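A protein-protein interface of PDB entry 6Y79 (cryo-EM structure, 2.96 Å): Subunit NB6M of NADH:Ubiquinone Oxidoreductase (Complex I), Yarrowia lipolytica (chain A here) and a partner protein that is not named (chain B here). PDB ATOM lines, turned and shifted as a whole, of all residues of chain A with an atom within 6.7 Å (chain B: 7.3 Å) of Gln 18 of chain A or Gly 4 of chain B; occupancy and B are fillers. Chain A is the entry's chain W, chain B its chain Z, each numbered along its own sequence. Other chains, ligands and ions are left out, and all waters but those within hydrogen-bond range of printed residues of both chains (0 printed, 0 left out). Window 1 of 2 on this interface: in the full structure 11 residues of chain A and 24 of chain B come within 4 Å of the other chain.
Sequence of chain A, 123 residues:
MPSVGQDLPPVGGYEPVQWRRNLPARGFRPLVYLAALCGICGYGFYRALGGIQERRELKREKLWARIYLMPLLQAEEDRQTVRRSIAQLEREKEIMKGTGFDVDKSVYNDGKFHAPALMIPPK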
ATOM      1  N   PRO A  16     -26.125  17.983  15.398  1.00  0.00           N
ATOM      2  CA  PRO A  16     -26.074  16.690  16.104  1.00  0.00           C
ATOM      3  C   PRO A  16     -24.846  16.512  16.990  1.00  0.00           C
ATOM      4  O   PRO A  16     -23.730  16.881  16.621  1.00  0.00           O
ATOM      5  CB  PRO A  16     -26.071  15.669  14.962  1.00  0.00           C
ATOM      6  CG  PRO A  16     -25.558  16.419  13.792  1.00  0.00           C
ATOM      7  CD  PRO A  16     -26.156  17.767  13.938  1.00  0.00           C
ATOM      8  N   VAL A  17     -25.073  15.957  18.182  1.00  0.00           N
ATOM      9  CA  VAL A  17     -23.991  15.573  19.084  1.00  0.00           C
ATOM     10  C   VAL A  17     -23.534  14.163  18.758  1.00  0.00           C
ATOM     11  O   VAL A  17     -24.147  13.461  17.950  1.00  0.00           O
ATOM     12  CB  VAL A  17     -24.381  15.649  20.568  1.00  0.00           C
ATOM     13  CG1 VAL A  17     -24.975  16.943  20.902  1.00  0.00           C
ATOM     14  CG2 VAL A  17     -25.350  14.588  20.891  1.00  0.00           C
ATOM     15  N   GLN A  18     -22.446  13.758  19.390  1.00  0.00           N
ATOM     16  CA  GLN A  18     -21.779  12.490  19.143  1.00  0.00           C
ATOM     17  C   GLN A  18     -22.291  11.419  20.102  1.00  0.00           C
ATOM     18  O   GLN A  18     -22.018  11.475  21.304  1.00  0.00           O
ATOM     19  CB  GLN A  18     -20.283  12.706  19.306  1.00  0.00           C
ATOM     20  CG  GLN A  18     -19.450  11.490  19.208  1.00  0.00           C
ATOM     21  CD  GLN A  18     -17.999  11.835  19.310  1.00  0.00           C
ATOM     22  OE1 GLN A  18     -17.636  12.941  19.703  1.00  0.00           O
ATOM     23  NE2 GLN A  18     -17.155  10.907  18.929  1.00  0.00           N
ATOM     24  N   TRP A  19     -23.020  10.435  19.572  1.00  0.00           N
ATOM     25  CA  TRP A  19     -23.455   9.294  20.369  1.00  0.00           C
ATOM     26  C   TRP A  19     -22.894   7.974  19.875  1.00  0.00           C
ATOM     27  O   TRP A  19     -23.304   6.926  20.371  1.00  0.00           O
ATOM     28  CB  TRP A  19     -24.981   9.190  20.419  1.00  0.00           C
ATOM     29  CG  TRP A  19     -25.663   9.026  19.113  1.00  0.00           C
ATOM     30  CD1 TRP A  19     -26.053  10.017  18.283  1.00  0.00           C
ATOM     31  CD2 TRP A  19     -26.074   7.800  18.498  1.00  0.00           C
ATOM     32  NE1 TRP A  19     -26.671   9.498  17.180  1.00  0.00           N
ATOM     33  CE2 TRP A  19     -26.695   8.135  17.287  1.00  0.00           C
ATOM     34  CE3 TRP A  19     -25.975   6.451  18.853  1.00  0.00           C
ATOM     35  CZ2 TRP A  19     -27.213   7.176  16.425  1.00  0.00           C
ATOM     36  CZ3 TRP A  19     -26.483   5.504  17.998  1.00  0.00           C
ATOM     37  CH2 TRP A  19     -27.100   5.868  16.801  1.00  0.00           C
ATOM     38  N   ARG A  20     -21.990   7.978  18.911  1.00  0.00           N
ATOM     39  CA  ARG A  20     -21.359   6.723  18.552  1.00  0.00           C
ATOM     40  C   ARG A  20     -20.163   6.486  19.457  1.00  0.00           C
ATOM     41  O   ARG A  20     -19.683   7.392  20.141  1.00  0.00           O
ATOM     42  CB  ARG A  20     -20.919   6.718  17.092  1.00  0.00           C
ATOM     43  CG  ARG A  20     -22.042   6.849  16.096  1.00  0.00           C
ATOM     44  CD  ARG A  20     -23.012   5.715  16.193  1.00  0.00           C
ATOM     45  NE  ARG A  20     -24.183   5.982  15.375  1.00  0.00           N
ATOM     46  CZ  ARG A  20     -24.354   5.516  14.149  1.00  0.00           C
ATOM     47  NH1 ARG A  20     -25.454   5.810  13.471  1.00  0.00           N
ATOM     48  NH2 ARG A  20     -23.424   4.752  13.606  1.00  0.00           N
ATOM     49  N   ARG A  21     -19.701   5.244  19.479  1.00  0.00           N
ATOM     50  CA  ARG A  21     -18.456   4.923  20.157  1.00  0.00           C
ATOM     51  C   ARG A  21     -17.294   5.522  19.385  1.00  0.00           C
ATOM     52  O   ARG A  21     -17.115   5.230  18.198  1.00  0.00           O
ATOM     53  CB  ARG A  21     -18.285   3.415  20.271  1.00  0.00           C
ATOM     54  CG  ARG A  21     -19.043   2.778  21.399  1.00  0.00           C
ATOM     55  CD  ARG A  21     -18.977   1.283  21.260  1.00  0.00           C
ATOM     56  NE  ARG A  21     -17.877   0.687  22.002  1.00  0.00           N
ATOM     57  CZ  ARG A  21     -17.157  -0.343  21.569  1.00  0.00           C
ATOM     58  NH1 ARG A  21     -16.192  -0.835  22.324  1.00  0.00           N
ATOM     59  NH2 ARG A  21     -17.393  -0.875  20.374  1.00  0.00           N
ATOM     60  N   ASN A  22     -16.513   6.370  20.043  1.00  0.00           N
ATOM     61  CA  ASN A  22     -15.302   6.925  19.451  1.00  0.00           C
ATOM     62  C   ASN A  22     -14.120   6.196  20.070  1.00  0.00           C
ATOM     63  O   ASN A  22     -13.440   6.713  20.954  1.00  0.00           O
ATOM     64  CB  ASN A  22     -15.204   8.383  19.686  1.00  0.00           C
ATOM     65  CG  ASN A  22     -14.195   9.048  18.788  1.00  0.00           C
ATOM     66  OD1 ASN A  22     -13.575   8.404  17.946  1.00  0.00           O
ATOM     67  ND2 ASN A  22     -14.026  10.349  18.958  1.00  0.00           N
ATOM     68  N   LEU B   2     -22.599   7.103  11.745  1.00  0.00           N
ATOM     69  CA  LEU B   2     -22.120   8.176  10.857  1.00  0.00           C
ATOM     70  C   LEU B   2     -23.015   9.446  10.737  1.00  0.00           C
ATOM     71  O   LEU B   2     -22.521  10.474  10.264  1.00  0.00           O
ATOM     72  CB  LEU B   2     -21.830   7.574   9.468  1.00  0.00           C
ATOM     73  CG  LEU B   2     -20.999   8.290   8.395  1.00  0.00           C
ATOM     74  CD1 LEU B   2     -20.014   7.327   7.727  1.00  0.00           C
ATOM     75  CD2 LEU B   2     -21.889   8.925   7.327  1.00  0.00           C
ATOM     76  N   PRO B   3     -24.321   9.441  11.166  1.00  0.00           N
ATOM     77  CA  PRO B   3     -24.931  10.740  11.491  1.00  0.00           C
ATOM     78  C   PRO B   3     -24.535  11.200  12.886  1.00  0.00           C
ATOM     79  O   PRO B   3     -24.403  12.400  13.138  1.00  0.00           O
ATOM     80  CB  PRO B   3     -26.438  10.474  11.370  1.00  0.00           C
ATOM     81  CG  PRO B   3     -26.586   9.045  11.566  1.00  0.00           C
ATOM     82  CD  PRO B   3     -25.375   8.437  10.934  1.00  0.00           C
ATOM     83  N   GLY B   4     -24.289  10.250  13.782  1.00  0.00           N
ATOM     84  CA  GLY B   4     -23.851  10.581  15.121  1.00  0.00           C
ATOM     85  C   GLY B   4     -22.387  10.282  15.378  1.00  0.00           C
ATOM     86  O   GLY B   4     -21.985  10.101  16.530  1.00  0.00           O
ATOM     87  N   GLY B   5     -21.577  10.249  14.319  1.00  0.00           N
ATOM     88  CA  GLY B   5     -20.192   9.842  14.409  1.00  0.00           C
ATOM     89  C   GLY B   5     -19.276  10.862  15.060  1.00  0.00           C
ATOM     90  O   GLY B   5     -19.725  11.801  15.723  1.00  0.00           O
ATOM     91  N   PRO B   6     -17.962  10.685  14.888  1.00  0.00           N
ATOM     92  CA  PRO B   6     -16.996  11.566  15.559  1.00  0.00           C
ATOM     93  C   PRO B   6     -17.013  12.978  14.995  1.00  0.00           C
ATOM     94  O   PRO B   6     -16.908  13.184  13.785  1.00  0.00           O
ATOM     95  CB  PRO B   6     -15.650  10.879  15.300  1.00  0.00           C
ATOM     96  CG  PRO B   6     -15.998   9.461  14.995  1.00  0.00           C
ATOM     97  CD  PRO B   6     -17.295   9.534  14.256  1.00  0.00           C
ATOM     98  N   VAL B   7     -17.150  13.951  15.891  1.00  0.00           N
ATOM     99  CA  VAL B   7     -17.119  15.365  15.532  1.00  0.00           C
ATOM    100  C   VAL B   7     -15.828  15.944  16.111  1.00  0.00           C
ATOM    101  O   VAL B   7     -15.314  15.416  17.106  1.00  0.00           O
ATOM    102  CB  VAL B   7     -18.389  16.087  16.022  1.00  0.00           C
ATOM    103  CG1 VAL B   7     -19.622  15.291  15.657  1.00  0.00           C
ATOM    104  CG2 VAL B   7     -18.371  16.302  17.512  1.00  0.00           C
ATOM    105  N   PRO B   8     -15.229  16.965  15.500  1.00  0.00           N
ATOM    106  CA  PRO B   8     -13.978  17.515  16.038  1.00  0.00           C
ATOM    107  C   PRO B   8     -14.234  18.379  17.262  1.00  0.00           C
ATOM    108  O   PRO B   8     -15.345  18.857  17.492  1.00  0.00           O
ATOM    109  CB  PRO B   8     -13.431  18.346  14.875  1.00  0.00           C
ATOM    110  CG  PRO B   8     -14.633  18.702  14.077  1.00  0.00           C
ATOM    111  CD  PRO B   8     -15.576  17.558  14.196  1.00  0.00           C
ATOM    112  N   LYS B  12     -17.895  21.446  20.651  1.00  0.00           N
ATOM    113  CA  LYS B  12     -18.226  20.649  21.824  1.00  0.00           C
ATOM    114  C   LYS B  12     -18.370  21.430  23.125  1.00  0.00           C
ATOM    115  O   LYS B  12     -18.693  20.809  24.144  1.00  0.00           O
ATOM    116  CB  LYS B  12     -17.187  19.538  22.035  1.00  0.00           C
ATOM    117  CG  LYS B  12     -17.348  18.300  21.155  1.00  0.00           C
ATOM    118  CD  LYS B  12     -16.184  17.365  21.427  1.00  0.00           C
ATOM    119  CE  LYS B  12     -16.121  16.181  20.488  1.00  0.00           C
ATOM    120  NZ  LYS B  12     -17.252  15.252  20.630  1.00  0.00           N
ATOM    121  N   ASN B  33     -10.071  14.387  18.975  1.00  0.00           N
ATOM    122  CA  ASN B  33     -11.355  15.076  19.082  1.00  0.00           C
ATOM    123  C   ASN B  33     -12.053  14.785  20.408  1.00  0.00           C
ATOM    124  O   ASN B  33     -13.220  14.408  20.454  1.00  0.00           O
ATOM    125  CB  ASN B  33     -12.242  14.718  17.893  1.00  0.00           C
ATOM    126  CG  ASN B  33     -12.454  13.220  17.723  1.00  0.00           C
ATOM    127  OD1 ASN B  33     -11.980  12.405  18.511  1.00  0.00           O
ATOM    128  ND2 ASN B  33     -13.191  12.856  16.683  1.00  0.00           N
ATOM    129  N   ARG B  34     -11.338  14.978  21.509  1.00  0.00           N
ATOM    130  CA  ARG B  34     -11.865  14.704  22.836  1.00  0.00           C
ATOM    131  C   ARG B  34     -11.795  15.960  23.685  1.00  0.00           C
ATOM    132  O   ARG B  34     -10.768  16.645  23.708  1.00  0.00           O
ATOM    133  CB  ARG B  34     -11.100  13.570  23.511  1.00  0.00           C
ATOM    134  CG  ARG B  34     -11.522  12.203  23.045  1.00  0.00           C
ATOM    135  CD  ARG B  34     -10.814  11.112  23.814  1.00  0.00           C
ATOM    136  NE  ARG B  34     -10.997   9.824  23.161  1.00  0.00           N
ATOM    137  CZ  ARG B  34     -10.331   8.721  23.471  1.00  0.00           C
ATOM    138  NH1 ARG B  34      -9.433   8.725  24.444  1.00  0.00           N
ATOM    139  NH2 ARG B  34     -10.574   7.603  22.805  1.00  0.00           N
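The side-chain amide oxygen (OE1) of Gln 18 of chain A lies within hydrogen-bond range of the side-chain amino group (NZ) of Lys 12 of chain B (2.5 Å). The backbone NH of Trp 19 of chain A lies within hydrogen-bond range of the backbone carbonyl oxygen of Gly 4 of chain B (3.2 Å). N of Arg 20 of chain A is in hydrogen-bond range of O of Gly 4 of chain B (3.2 Å). OD1 of Asn 33 of chain B is in hydrogen-bond range of ND2 of Asn 22 of chain A, at 2.9 Å. NH2 of Arg 20 of chain A lies close to N of Leu 2 of chain B (3.1 Å).
Gln 18 of chain A touches just these residues of chain B: Gly 4, Gly 5, Pro 6, Val 7 and Lys 12. Printed residues of chain B within 4 Å of Trp 19 of chain A: Gly 4 (3.2 Å). Printed residues of chain B within 4 Å of Asn 22 of chain A: Pro 6 (3.96 Å), Asn 33 (2.9 Å) and Arg 34 (3.5 Å). Of the printed residues of chain A, Pro 3 of chain B touches Arg 20 (3.7 Å). Gly 4 of chain B touches three residues of chain A. Of the printed residues of chain A, Asn 33 of chain B touches Asn 22 (2.9 Å). Of the printed residues of chain A, Arg 34 of chain B touches Asn 22.
Among the printed residues, merely in contact across the chains: Gln 18 of chain A with Pro 6 of chain B, Gln 18 of chain A with Gly 5 of chain B, Asn 22 of chain A with Arg 34 of chain B, Gln 18 of chain A with Gly 4 of chain B, Arg 20 of chain A with Pro 3 of chain B, Arg 20 of chain A with Gly 5 of chain B, Asn 22 of chain A with Pro 6 of chain B and Gln 18 of chain A with Val 7 of chain B.
Printed residues of chain B that touch a printed residue of chain A: Leu 2, Pro 3, Gly 4, Gly 5, Pro 6, Val 7, Lys 12, Asn 33 and Arg 34. Hydrophobic or aromatic side chains of chain B within 4 Å of the printed part of chain A: Pro 3 and Pro 6. Hydrophobic or aromatic side chains of chain A within 4 Å of the printed part of chain B: Trp 19.
The side-chain amide nitrogen (ND2) of Asn 33 of chain B sits close to the backbone carbonyl oxygen (O) of Val 7 of chain B, at 3.4 Å. The side-chain amide nitrogen (ND2) of Asn 22 of chain A sits close to the side-chain amide nitrogen (NE2) of Gln 18 of chain A (3.2 Å).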
